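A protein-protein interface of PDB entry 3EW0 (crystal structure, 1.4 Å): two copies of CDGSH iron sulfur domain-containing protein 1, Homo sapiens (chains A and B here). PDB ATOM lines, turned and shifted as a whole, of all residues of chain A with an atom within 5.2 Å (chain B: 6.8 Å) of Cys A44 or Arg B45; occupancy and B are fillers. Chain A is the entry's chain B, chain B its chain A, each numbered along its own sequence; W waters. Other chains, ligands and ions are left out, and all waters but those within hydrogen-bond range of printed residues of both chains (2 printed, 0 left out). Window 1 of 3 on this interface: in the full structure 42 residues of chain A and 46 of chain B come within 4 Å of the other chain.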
ATOM      1  N   ILE A  17      -6.435  -0.026 -28.511  1.00  0.00           N
ATOM      2  CA  ILE A  17      -5.969   1.075 -27.674  1.00  0.00           C
ATOM      3  C   ILE A  17      -6.636   0.994 -26.295  1.00  0.00           C
ATOM      4  O   ILE A  17      -5.966   1.053 -25.259  1.00  0.00           O
ATOM      5  CB  ILE A  17      -6.307   2.419 -28.321  1.00  0.00           C
ATOM      6  CG1 ILE A  17      -5.366   2.692 -29.506  1.00  0.00           C
ATOM      7  CG2 ILE A  17      -6.211   3.498 -27.284  1.00  0.00           C
ATOM      8  CD1 ILE A  17      -5.874   3.816 -30.436  1.00  0.00           C
ATOM      9  N   ILE A  28     -17.029   4.883 -27.892  1.00  0.00           N
ATOM     10  CA  ILE A  28     -17.031   5.710 -26.697  1.00  0.00           C
ATOM     11  C   ILE A  28     -16.683   7.159 -26.999  1.00  0.00           C
ATOM     12  O   ILE A  28     -15.558   7.471 -27.366  1.00  0.00           O
ATOM     13  CB  ILE A  28     -16.054   5.161 -25.662  1.00  0.00           C
ATOM     14  CG1 ILE A  28     -16.466   3.761 -25.218  1.00  0.00           C
ATOM     15  CG2 ILE A  28     -15.996   6.091 -24.438  1.00  0.00           C
ATOM     16  CD1 ILE A  28     -15.332   3.045 -24.494  1.00  0.00           C
ATOM     17  N   VAL A  29     -17.688   8.002 -26.838  1.00  0.00           N
ATOM     18  CA  VAL A  29     -17.574   9.454 -26.991  1.00  0.00           C
ATOM     19  C   VAL A  29     -18.074  10.143 -25.725  1.00  0.00           C
ATOM     20  O   VAL A  29     -19.079   9.757 -25.155  1.00  0.00           O
ATOM     21  CB  VAL A  29     -18.444   9.983 -28.179  1.00  0.00           C
ATOM     22  CG1 VAL A  29     -18.325  11.542 -28.344  1.00  0.00           C
ATOM     23  CG2 VAL A  29     -18.079   9.290 -29.487  1.00  0.00           C
ATOM     24  N   HIS A  30     -17.347  11.145 -25.260  1.00  0.00           N
ATOM     25  CA  HIS A  30     -17.810  11.961 -24.151  1.00  0.00           C
ATOM     26  C   HIS A  30     -17.968  13.368 -24.644  1.00  0.00           C
ATOM     27  O   HIS A  30     -17.123  13.873 -25.383  1.00  0.00           O
ATOM     28  CB  HIS A  30     -16.798  11.946 -23.018  1.00  0.00           C
ATOM     29  CG  HIS A  30     -16.723  10.646 -22.301  1.00  0.00           C
ATOM     30  ND1 HIS A  30     -15.941   9.606 -22.749  1.00  0.00           N
ATOM     31  CD2 HIS A  30     -17.345  10.203 -21.183  1.00  0.00           C
ATOM     32  CE1 HIS A  30     -16.077   8.579 -21.932  1.00  0.00           C
ATOM     33  NE2 HIS A  30     -16.922   8.912 -20.971  1.00  0.00           N
ATOM     34  N   VAL A  42      -8.930  17.710 -16.746  1.00  0.00           N
ATOM     35  CA  VAL A  42      -7.835  17.007 -17.403  1.00  0.00           C
ATOM     36  C   VAL A  42      -8.344  15.651 -17.876  1.00  0.00           C
ATOM     37  O   VAL A  42      -8.812  14.851 -17.070  1.00  0.00           O
ATOM     38  CB  VAL A  42      -6.620  16.797 -16.466  1.00  0.00           C
ATOM     39  CG1 VAL A  42      -5.428  16.210 -17.251  1.00  0.00           C
ATOM     40  CG2 VAL A  42      -6.245  18.122 -15.755  1.00  0.00           C
ATOM     41  N   TYR A  43      -8.313  15.458 -19.181  1.00  0.00           N
ATOM     42  CA  TYR A  43      -8.937  14.295 -19.831  1.00  0.00           C
ATOM     43  C   TYR A  43      -7.905  13.299 -20.309  1.00  0.00           C
ATOM     44  O   TYR A  43      -6.888  13.661 -20.878  1.00  0.00           O
ATOM     45  CB  TYR A  43      -9.826  14.753 -21.004  1.00  0.00           C
ATOM     46  CG  TYR A  43     -10.965  15.644 -20.589  1.00  0.00           C
ATOM     47  CD1 TYR A  43     -12.122  15.121 -20.033  1.00  0.00           C
ATOM     48  CD2 TYR A  43     -10.858  17.026 -20.694  1.00  0.00           C
ATOM     49  CE1 TYR A  43     -13.158  15.956 -19.642  1.00  0.00           C
ATOM     50  CE2 TYR A  43     -11.917  17.883 -20.293  1.00  0.00           C
ATOM     51  CZ  TYR A  43     -13.050  17.322 -19.765  1.00  0.00           C
ATOM     52  OH  TYR A  43     -14.075  18.137 -19.352  1.00  0.00           O
ATOM     53  N   CYS A  44      -8.177  12.040 -20.047  1.00  0.00           N
ATOM     54  CA  CYS A  44      -7.313  10.937 -20.446  1.00  0.00           C
ATOM     55  C   CYS A  44      -7.374  10.666 -21.938  1.00  0.00           C
ATOM     56  O   CYS A  44      -8.441  10.599 -22.567  1.00  0.00           O
ATOM     57  CB  CYS A  44      -7.719   9.690 -19.693  1.00  0.00           C
ATOM     58  SG  CYS A  44      -6.798   8.190 -20.055  1.00  0.00           S
ATOM     59  N   ARG A  45      -6.194  10.603 -22.531  1.00  0.00           N
ATOM     60  CA  ARG A  45      -6.093  10.169 -23.911  1.00  0.00           C
ATOM     61  C   ARG A  45      -5.343   8.819 -24.092  1.00  0.00           C
ATOM     62  O   ARG A  45      -4.972   8.483 -25.203  1.00  0.00           O
ATOM     63  CB  ARG A  45      -5.397  11.257 -24.711  1.00  0.00           C
ATOM     64  CG  ARG A  45      -6.134  12.591 -24.704  1.00  0.00           C
ATOM     65  CD  ARG A  45      -5.585  13.556 -25.710  1.00  0.00           C
ATOM     66  NE  ARG A  45      -4.242  14.029 -25.373  1.00  0.00           N
ATOM     67  CZ  ARG A  45      -3.643  15.081 -25.947  1.00  0.00           C
ATOM     68  NH1 ARG A  45      -4.251  15.786 -26.889  1.00  0.00           N
ATOM     69  NH2 ARG A  45      -2.424  15.433 -25.577  1.00  0.00           N
ATOM     70  N   CYS A  46      -5.131   8.074 -23.002  1.00  0.00           N
ATOM     71  CA  CYS A  46      -4.381   6.792 -23.020  1.00  0.00           C
ATOM     72  C   CYS A  46      -5.259   5.570 -22.717  1.00  0.00           C
ATOM     73  O   CYS A  46      -4.818   4.432 -22.926  1.00  0.00           O
ATOM     74  CB  CYS A  46      -3.194   6.893 -22.055  1.00  0.00           C
ATOM     75  SG  CYS A  46      -3.587   6.665 -20.300  1.00  0.00           S
ATOM     76  N   TRP A  47      -6.495   5.816 -22.266  1.00  0.00           N
ATOM     77  CA  TRP A  47      -7.490   4.771 -21.949  1.00  0.00           C
ATOM     78  C   TRP A  47      -7.022   3.853 -20.814  1.00  0.00           C
ATOM     79  O   TRP A  47      -7.515   2.728 -20.670  1.00  0.00           O
ATOM     80  CB  TRP A  47      -7.879   3.958 -23.202  1.00  0.00           C
ATOM     81  CG  TRP A  47      -8.434   4.867 -24.238  1.00  0.00           C
ATOM     82  CD1 TRP A  47      -7.719   5.673 -25.071  1.00  0.00           C
ATOM     83  CD2 TRP A  47      -9.822   5.129 -24.516  1.00  0.00           C
ATOM     84  NE1 TRP A  47      -8.571   6.402 -25.862  1.00  0.00           N
ATOM     85  CE2 TRP A  47      -9.864   6.095 -25.540  1.00  0.00           C
ATOM     86  CE3 TRP A  47     -11.029   4.640 -24.006  1.00  0.00           C
ATOM     87  CZ2 TRP A  47     -11.078   6.582 -26.066  1.00  0.00           C
ATOM     88  CZ3 TRP A  47     -12.213   5.119 -24.534  1.00  0.00           C
ATOM     89  CH2 TRP A  47     -12.226   6.067 -25.546  1.00  0.00           C
ATOM     90  N   ARG A  48      -6.118   4.369 -19.975  1.00  0.00           N
ATOM     91  CA  ARG A  48      -5.542   3.553 -18.889  1.00  0.00           C
ATOM     92  C   ARG A  48      -6.016   4.060 -17.542  1.00  0.00           C
ATOM     93  O   ARG A  48      -5.896   3.385 -16.529  1.00  0.00           O
ATOM     94  CB  ARG A  48      -4.011   3.545 -18.934  1.00  0.00           C
ATOM     95  CG  ARG A  48      -3.412   2.953 -20.204  1.00  0.00           C
ATOM     96  CD  ARG A  48      -3.592   1.460 -20.274  1.00  0.00           C
ATOM     97  NE  ARG A  48      -3.095   0.887 -21.530  1.00  0.00           N
ATOM     98  CZ  ARG A  48      -3.748   0.884 -22.695  1.00  0.00           C
ATOM     99  NH1 ARG A  48      -4.939   1.448 -22.813  1.00  0.00           N
ATOM    100  NH2 ARG A  48      -3.195   0.306 -23.763  1.00  0.00           N
ATOM    101  N   SER A  49      -6.575   5.263 -17.521  1.00  0.00           N
ATOM    102  CA  SER A  49      -6.998   5.866 -16.279  1.00  0.00           C
ATOM    103  C   SER A  49      -8.058   5.037 -15.606  1.00  0.00           C
ATOM    104  O   SER A  49      -8.974   4.549 -16.261  1.00  0.00           O
ATOM    105  CB  SER A  49      -7.562   7.253 -16.544  1.00  0.00           C
ATOM    106  OG  SER A  49      -8.018   7.815 -15.347  1.00  0.00           O
ATOM    107  N   PHE A  52     -11.310   7.187 -16.036  1.00  0.00           N
ATOM    108  CA  PHE A  52     -11.660   7.579 -17.394  1.00  0.00           C
ATOM    109  C   PHE A  52     -13.095   8.085 -17.402  1.00  0.00           C
ATOM    110  O   PHE A  52     -13.957   7.465 -16.786  1.00  0.00           O
ATOM    111  CB  PHE A  52     -11.519   6.397 -18.361  1.00  0.00           C
ATOM    112  CG  PHE A  52     -11.484   6.807 -19.798  1.00  0.00           C
ATOM    113  CD1 PHE A  52     -10.283   7.217 -20.397  1.00  0.00           C
ATOM    114  CD2 PHE A  52     -12.645   6.817 -20.557  1.00  0.00           C
ATOM    115  CE1 PHE A  52     -10.245   7.606 -21.727  1.00  0.00           C
ATOM    116  CE2 PHE A  52     -12.608   7.219 -21.880  1.00  0.00           C
ATOM    117  CZ  PHE A  52     -11.405   7.627 -22.461  1.00  0.00           C
ATOM    118  N   PRO A  53     -13.365   9.204 -18.099  1.00  0.00           N
ATOM    119  CA  PRO A  53     -12.510   9.910 -19.052  1.00  0.00           C
ATOM    120  C   PRO A  53     -11.468  10.900 -18.490  1.00  0.00           C
ATOM    121  O   PRO A  53     -10.842  11.650 -19.285  1.00  0.00           O
ATOM    122  CB  PRO A  53     -13.544  10.690 -19.875  1.00  0.00           C
ATOM    123  CG  PRO A  53     -14.583  11.057 -18.900  1.00  0.00           C
ATOM    124  CD  PRO A  53     -14.689   9.855 -17.995  1.00  0.00           C
ATOM    125  N   PHE A  54     -11.266  10.894 -17.177  1.00  0.00           N
ATOM    126  CA  PHE A  54     -10.371  11.850 -16.531  1.00  0.00           C
ATOM    127  C   PHE A  54      -9.000  11.205 -16.341  1.00  0.00           C
ATOM    128  O   PHE A  54      -8.901  10.000 -16.074  1.00  0.00           O
ATOM    129  CB  PHE A  54     -10.993  12.330 -15.206  1.00  0.00           C
ATOM    130  CG  PHE A  54     -12.385  12.858 -15.372  1.00  0.00           C
ATOM    131  CD1 PHE A  54     -12.587  14.087 -15.977  1.00  0.00           C
ATOM    132  CD2 PHE A  54     -13.490  12.128 -14.952  1.00  0.00           C
ATOM    133  CE1 PHE A  54     -13.850  14.578 -16.169  1.00  0.00           C
ATOM    134  CE2 PHE A  54     -14.756  12.610 -15.144  1.00  0.00           C
ATOM    135  CZ  PHE A  54     -14.947  13.840 -15.756  1.00  0.00           C
ATOM    136  N   CYS A  55      -7.963  12.025 -16.501  1.00  0.00           N
ATOM    137  CA  CYS A  55      -6.569  11.606 -16.322  1.00  0.00           C
ATOM    138  C   CYS A  55      -6.256  11.439 -14.846  1.00  0.00           C
ATOM    139  O   CYS A  55      -6.471  12.341 -14.057  1.00  0.00           O
ATOM    140  CB  CYS A  55      -5.617  12.641 -16.938  1.00  0.00           C
ATOM    141  SG  CYS A  55      -3.866  12.283 -16.715  1.00  0.00           S
ATOM    142  N   PRO A  72      -2.281  13.787 -21.450  1.00  0.00           N
ATOM    143  CA  PRO A  72      -3.682  14.242 -21.391  1.00  0.00           C
ATOM    144  C   PRO A  72      -3.985  15.542 -22.108  1.00  0.00           C
ATOM    145  O   PRO A  72      -3.109  16.227 -22.626  1.00  0.00           O
ATOM    146  CB  PRO A  72      -3.916  14.429 -19.894  1.00  0.00           C
ATOM    147  CG  PRO A  72      -2.558  14.754 -19.347  1.00  0.00           C
ATOM    148  CD  PRO A  72      -1.598  13.922 -20.149  1.00  0.00           C
ATOM    149  N   ILE B  17       0.348   3.281 -28.004  1.00  0.00           N
ATOM    150  CA  ILE B  17      -0.927   3.802 -28.479  1.00  0.00           C
ATOM    151  C   ILE B  17      -0.696   4.796 -29.614  1.00  0.00           C
ATOM    152  O   ILE B  17      -1.358   4.763 -30.649  1.00  0.00           O
ATOM    153  CB  ILE B  17      -1.706   4.473 -27.313  1.00  0.00           C
ATOM    154  CG1 ILE B  17      -2.204   3.400 -26.337  1.00  0.00           C
ATOM    155  CG2 ILE B  17      -2.860   5.326 -27.829  1.00  0.00           C
ATOM    156  CD1 ILE B  17      -2.743   3.965 -25.009  1.00  0.00           C
ATOM    157  N   TYR B  43     -11.821  16.476 -29.921  1.00  0.00           N
ATOM    158  CA  TYR B  43     -10.441  16.133 -29.651  1.00  0.00           C
ATOM    159  C   TYR B  43     -10.213  14.626 -29.822  1.00  0.00           C
ATOM    160  O   TYR B  43     -11.011  13.794 -29.386  1.00  0.00           O
ATOM    161  CB  TYR B  43     -10.092  16.543 -28.236  1.00  0.00           C
ATOM    162  CG  TYR B  43     -10.181  18.024 -27.993  1.00  0.00           C
ATOM    163  CD1 TYR B  43      -9.261  18.890 -28.567  1.00  0.00           C
ATOM    164  CD2 TYR B  43     -11.185  18.566 -27.200  1.00  0.00           C
ATOM    165  CE1 TYR B  43      -9.359  20.257 -28.360  1.00  0.00           C
ATOM    166  CE2 TYR B  43     -11.275  19.921 -26.968  1.00  0.00           C
ATOM    167  CZ  TYR B  43     -10.356  20.760 -27.547  1.00  0.00           C
ATOM    168  OH  TYR B  43     -10.454  22.125 -27.312  1.00  0.00           O
ATOM    169  N   CYS B  44      -9.110  14.292 -30.462  1.00  0.00           N
ATOM    170  CA  CYS B  44      -8.752  12.915 -30.757  1.00  0.00           C
ATOM    171  C   CYS B  44      -8.229  12.180 -29.501  1.00  0.00           C
ATOM    172  O   CYS B  44      -7.417  12.723 -28.742  1.00  0.00           O
ATOM    173  CB  CYS B  44      -7.710  12.918 -31.863  1.00  0.00           C
ATOM    174  SG  CYS B  44      -7.035  11.311 -32.273  1.00  0.00           S
ATOM    175  N   ARG B  45      -8.709  10.951 -29.275  1.00  0.00           N
ATOM    176  CA  ARG B  45      -8.259  10.090 -28.204  1.00  0.00           C
ATOM    177  C   ARG B  45      -7.697   8.775 -28.746  1.00  0.00           C
ATOM    178  O   ARG B  45      -7.470   7.853 -27.986  1.00  0.00           O
ATOM    179  CB  ARG B  45      -9.384   9.842 -27.172  1.00  0.00           C
ATOM    180  CG  ARG B  45      -9.877  11.109 -26.435  1.00  0.00           C
ATOM    181  CD  ARG B  45     -10.805  10.779 -25.284  1.00  0.00           C
ATOM    182  NE  ARG B  45     -12.052  10.164 -25.701  1.00  0.00           N
ATOM    183  CZ  ARG B  45     -13.098   9.978 -24.898  1.00  0.00           C
ATOM    184  NH1 ARG B  45     -13.092  10.462 -23.648  1.00  0.00           N
ATOM    185  NH2 ARG B  45     -14.187   9.362 -25.355  1.00  0.00           N
ATOM    186  N   CYS B  46      -7.462   8.708 -30.047  1.00  0.00           N
ATOM    187  CA  CYS B  46      -6.949   7.480 -30.682  1.00  0.00           C
ATOM    188  C   CYS B  46      -5.513   7.645 -31.235  1.00  0.00           C
ATOM    189  O   CYS B  46      -4.896   6.678 -31.632  1.00  0.00           O
ATOM    190  CB  CYS B  46      -7.902   7.036 -31.818  1.00  0.00           C
ATOM    191  SG  CYS B  46      -7.766   8.015 -33.338  1.00  0.00           S
ATOM    192  N   TRP B  47      -5.000   8.863 -31.299  1.00  0.00           N
ATOM    193  CA  TRP B  47      -3.624   9.123 -31.779  1.00  0.00           C
ATOM    194  C   TRP B  47      -3.373   8.674 -33.226  1.00  0.00           C
ATOM    195  O   TRP B  47      -2.256   8.276 -33.588  1.00  0.00           O
ATOM    196  CB  TRP B  47      -2.558   8.522 -30.823  1.00  0.00           C
ATOM    197  CG  TRP B  47      -2.732   9.066 -29.444  1.00  0.00           C
ATOM    198  CD1 TRP B  47      -3.626   8.635 -28.512  1.00  0.00           C
ATOM    199  CD2 TRP B  47      -2.031  10.173 -28.858  1.00  0.00           C
ATOM    200  NE1 TRP B  47      -3.523   9.402 -27.381  1.00  0.00           N
ATOM    201  CE2 TRP B  47      -2.562  10.358 -27.566  1.00  0.00           C
ATOM    202  CE3 TRP B  47      -1.019  11.030 -29.305  1.00  0.00           C
ATOM    203  CZ2 TRP B  47      -2.120  11.363 -26.703  1.00  0.00           C
ATOM    204  CZ3 TRP B  47      -0.566  12.042 -28.442  1.00  0.00           C
ATOM    205  CH2 TRP B  47      -1.115  12.191 -27.153  1.00  0.00           C
ATOM    206  N   ARG B  48      -4.426   8.732 -34.037  1.00  0.00           N
ATOM    207  CA  ARG B  48      -4.334   8.439 -35.475  1.00  0.00           C
ATOM    208  C   ARG B  48      -4.712   9.616 -36.354  1.00  0.00           C
ATOM    209  O   ARG B  48      -4.435   9.590 -37.555  1.00  0.00           O
ATOM    210  CB  ARG B  48      -5.190   7.229 -35.902  1.00  0.00           C
ATOM    211  CG  ARG B  48      -4.969   5.926 -35.132  1.00  0.00           C
ATOM    212  CD  ARG B  48      -3.729   5.196 -35.535  1.00  0.00           C
ATOM    213  NE  ARG B  48      -3.530   3.998 -34.712  1.00  0.00           N
ATOM    214  CZ  ARG B  48      -2.918   3.976 -33.525  1.00  0.00           C
ATOM    215  NH1 ARG B  48      -2.422   5.089 -32.997  1.00  0.00           N
ATOM    216  NH2 ARG B  48      -2.807   2.837 -32.852  1.00  0.00           N
ATOM    217  N   PHE B  52      -4.293  15.820 -35.344  1.00  0.00           N
ATOM    218  CA  PHE B  52      -4.066  15.751 -33.888  1.00  0.00           C
ATOM    219  C   PHE B  52      -3.617  17.111 -33.371  1.00  0.00           C
ATOM    220  O   PHE B  52      -2.683  17.684 -33.925  1.00  0.00           O
ATOM    221  CB  PHE B  52      -3.013  14.699 -33.524  1.00  0.00           C
ATOM    222  CG  PHE B  52      -3.090  14.271 -32.094  1.00  0.00           C
ATOM    223  CD1 PHE B  52      -4.002  13.296 -31.719  1.00  0.00           C
ATOM    224  CD2 PHE B  52      -2.316  14.888 -31.109  1.00  0.00           C
ATOM    225  CE1 PHE B  52      -4.137  12.913 -30.409  1.00  0.00           C
ATOM    226  CE2 PHE B  52      -2.444  14.496 -29.780  1.00  0.00           C
ATOM    227  CZ  PHE B  52      -3.355  13.505 -29.436  1.00  0.00           C
ATOM    228  N   PRO B  53      -4.220  17.600 -32.270  1.00  0.00           N
ATOM    229  CA  PRO B  53      -5.101  16.960 -31.282  1.00  0.00           C
ATOM    230  C   PRO B  53      -6.589  16.872 -31.634  1.00  0.00           C
ATOM    231  O   PRO B  53      -7.359  16.362 -30.823  1.00  0.00           O
ATOM    232  CB  PRO B  53      -4.945  17.878 -30.067  1.00  0.00           C
ATOM    233  CG  PRO B  53      -4.761  19.222 -30.641  1.00  0.00           C
ATOM    234  CD  PRO B  53      -3.954  19.005 -31.898  1.00  0.00           C
ATOM    235  N   CYS B  55      -9.896  15.512 -33.745  1.00  0.00           N
ATOM    236  CA  CYS B  55     -10.410  14.295 -34.385  1.00  0.00           C
ATOM    237  C   CYS B  55     -10.685  14.569 -35.867  1.00  0.00           C
ATOM    238  O   CYS B  55     -11.273  15.600 -36.210  1.00  0.00           O
ATOM    239  CB  CYS B  55     -11.728  13.904 -33.699  1.00  0.00           C
ATOM    240  SG  CYS B  55     -12.565  12.439 -34.367  1.00  0.00           S
ATOM    241  N   HIS B  59     -10.308   7.422 -36.051  1.00  0.00           N
ATOM    242  CA  HIS B  59     -10.683   6.390 -35.091  1.00  0.00           C
ATOM    243  C   HIS B  59     -11.515   5.261 -35.721  1.00  0.00           C
ATOM    244  O   HIS B  59     -11.368   4.098 -35.341  1.00  0.00           O
ATOM    245  CB  HIS B  59     -11.420   7.009 -33.900  1.00  0.00           C
ATOM    246  CG  HIS B  59     -12.643   7.775 -34.277  1.00  0.00           C
ATOM    247  ND1 HIS B  59     -12.666   9.155 -34.407  1.00  0.00           N
ATOM    248  CD2 HIS B  59     -13.900   7.339 -34.526  1.00  0.00           C
ATOM    249  CE1 HIS B  59     -13.891   9.520 -34.749  1.00  0.00           C
ATOM    250  NE2 HIS B  59     -14.655   8.442 -34.827  1.00  0.00           N
ATOM    251  N   VAL B  70     -12.962   3.044 -29.534  1.00  0.00           N
ATOM    252  CA  VAL B  70     -12.517   4.347 -29.081  1.00  0.00           C
ATOM    253  C   VAL B  70     -13.186   5.453 -29.894  1.00  0.00           C
ATOM    254  O   VAL B  70     -13.581   5.282 -31.043  1.00  0.00           O
ATOM    255  CB  VAL B  70     -10.945   4.489 -29.099  1.00  0.00           C
ATOM    256  CG1 VAL B  70     -10.301   3.558 -28.070  1.00  0.00           C
ATOM    257  CG2 VAL B  70     -10.369   4.280 -30.487  1.00  0.00           C
ATOM    258  N   GLY B  71     -13.318   6.608 -29.273  1.00  0.00           N
ATOM    259  CA  GLY B  71     -13.957   7.770 -29.895  1.00  0.00           C
ATOM    260  C   GLY B  71     -13.408   9.016 -29.224  1.00  0.00           C
ATOM    261  O   GLY B  71     -12.671   8.927 -28.225  1.00  0.00           O
ATOM    262  N   PRO B  72     -13.747  10.185 -29.768  1.00  0.00           N
ATOM    263  CA  PRO B  72     -13.214  11.480 -29.335  1.00  0.00           C
ATOM    264  C   PRO B  72     -13.848  12.059 -28.055  1.00  0.00           C
ATOM    265  O   PRO B  72     -14.826  11.518 -27.540  1.00  0.00           O
ATOM    266  CB  PRO B  72     -13.488  12.380 -30.537  1.00  0.00           C
ATOM    267  CG  PRO B  72     -14.704  11.759 -31.194  1.00  0.00           C
ATOM    268  CD  PRO B  72     -14.477  10.280 -31.045  1.00  0.00           C
ATOM    269  N   LEU B  73     -13.271  13.154 -27.559  1.00  0.00           N
ATOM    270  CA  LEU B  73     -13.798  13.926 -26.461  1.00  0.00           C
ATOM    271  C   LEU B  73     -14.287  15.229 -27.089  1.00  0.00           C
ATOM    272  O   LEU B  73     -13.567  15.877 -27.857  1.00  0.00           O
ATOM    273  CB  LEU B  73     -12.708  14.200 -25.418  1.00  0.00           C
ATOM    274  CG  LEU B  73     -13.082  15.291 -24.407  1.00  0.00           C
ATOM    275  CD1 LEU B  73     -13.974  14.725 -23.313  1.00  0.00           C
ATOM    276  CD2 LEU B  73     -11.841  15.945 -23.838  1.00  0.00           C
ATOM    277  N   ILE B  74     -15.506  15.613 -26.715  1.00  0.00           N
ATOM    278  CA  ILE B  74     -16.148  16.793 -27.235  1.00  0.00           C
ATOM    279  C   ILE B  74     -16.347  17.807 -26.122  1.00  0.00           C
ATOM    280  O   ILE B  74     -16.878  17.492 -25.048  1.00  0.00           O
ATOM    281  CB  ILE B  74     -17.499  16.421 -27.848  1.00  0.00           C
ATOM    282  CG1 ILE B  74     -17.312  15.552 -29.097  1.00  0.00           C
ATOM    283  CG2 ILE B  74     -18.272  17.656 -28.237  1.00  0.00           C
ATOM    284  CD1 ILE B  74     -18.561  14.862 -29.606  1.00  0.00           C
HETATM  285  O   HOH W   1      -6.692  15.294 -28.307  1.00  0.00           O
HETATM  286  O   HOH W   2     -10.956  11.545 -22.117  1.00  0.00           O
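The guanidinium group (NH2) of Arg B45 lies within hydrogen-bond range of the backbone carbonyl oxygen (O) of Ile A28. NH1 of Arg B45 is in hydrogen-bond range of ND1 of His A30 (3.1 Å). The backbone carbonyl oxygen of Arg B45 sits at hydrogen-bond distance from the indole nitrogen of Trp A47 (2.8 Å). The backbone carbonyl oxygen (O) of Arg A45 is in hydrogen-bond range of the indole nitrogen (NE1) of Trp B47 (2.8 Å). The backbone NH (N) of Gly B71 sits close to the backbone carbonyl oxygen (O) of Ile A28 (3.1 Å). The backbone NH (N) of His A30 lies within hydrogen-bond range of the backbone carbonyl oxygen (O) of Pro B72 (3.4 Å). The backbone carbonyl oxygen of His A30 is in hydrogen-bond range of the backbone NH of Ile B74 (2.7 Å).
Among the printed residues, pairs that only touch across the chains: Ile A17 with Ile B17 (3.9 Å), Ile A17 with Cys B46 (3.3 Å), Val A29 with Arg B45 (3.8 Å), Val A29 with Pro B72 (3.5 Å), Val A29 with Ile B74 (3.6 Å), His A30 with Leu B73 (3.5 Å), Tyr A43 with Leu B73 (3.4 Å), Cys A44 with Arg B45 (3.6 Å), Arg A45 with Cys B44 (3.6 Å), Arg A45 with Arg B45 (3.8 Å), Arg A45 with Phe B52 (3.5 Å), Arg A45 with Pro B53 (3.9 Å), Cys A46 with Ile B17 (3.0 Å), Trp A47 with Val B70 (3.6 Å), Trp A47 with Gly B71 (3.6 Å), Arg A48 with Ile B17 (3.9 Å), Phe A52 with Arg B45 (3.5 Å) and Pro A53 with Arg B45 (3.8 Å).
Ile B17 touches its own counterpart, Ile A17. Ile A17 touches Cys B46, and with the chains exchanged Cys A46 touches Ile B17. Arg A45 touches Phe B52, and with the chains exchanged Phe A52 touches Arg B45. Arg A48 touches Ile B17, but with the chains exchanged Ile A17 does not touch Arg B48 (4.03 Å). Positions printed for both chains: 17, 43, 44, 45, 46, 47, 48, 52, 53, 55 and 72.
Water W1 lies within hydrogen-bond range of the backbone carbonyl oxygen of Cys B44, the backbone carbonyl oxygen of Pro B53 and the guanidinium group of Arg A45. Water W2 lies within hydrogen-bond range of the backbone carbonyl oxygen of Cys A44 (2.7 Å), the backbone carbonyl oxygen of Pro A53 (2.8 Å) and the guanidinium group of Arg B45 (2.8 Å).
Of the 16 printed residues of chain B, 12 touch a printed residue of chain A. Along chain B the printed residues that touch a printed residue of chain A span positions 17 to 74. Hydrophobic or aromatic side chains of chain A within 4 Å of the printed part of chain B: Ile A17, Ile A28, Val A29, His A30, Tyr A43, Trp A47, Phe A52 and Pro A53.
Val A42 touches none of the printed residues of chain B. Printed residues of chain B within 4 Å of Tyr A43: Leu B73 (3.4 Å). Printed residues of chain B within 4 Å of Trp A47: Arg B45 (2.8 Å), Val B70 (3.6 Å) and Gly B71 (3.6 Å). Of the printed residues of chain B, Arg A48 touches Ile B17. Ser A49 touches none of the printed residues of chain B. Printed residues of chain B within 4 Å of Pro A53: Arg B45. Arg B45 touches just these residues of chain A: Ile A28, Val A29, His A30, Cys A44, Arg A45, Trp A47, Phe A52 and Pro A53. The nearest residue of chain B that does not touch Cys A44 is Leu B73 (6.3 Å). The nearest printed residue of chain B that does not touch Val A29 is Gly B71 (4.4 Å).
N of Tyr B43 is in hydrogen-bond range of O of Leu B73, 2.8 Å away. The backbone carbonyl oxygen of Cys B46 sits at hydrogen-bond distance from the guanidinium group of Arg B48 (3.2 Å). The backbone NH (N) of Cys A44 sits at hydrogen-bond distance from the backbone carbonyl oxygen (O) of Pro A53 (2.8 Å). O of Pro A72 is in hydrogen-bond range of NH2 of Arg A45. The backbone carbonyl oxygen of Cys A46 sits at hydrogen-bond distance from the guanidinium group of Arg A48. The side-chain hydroxyl (OG) of Ser A49 is in hydrogen-bond range of the backbone NH (N) of Phe A52 (3.4 Å).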
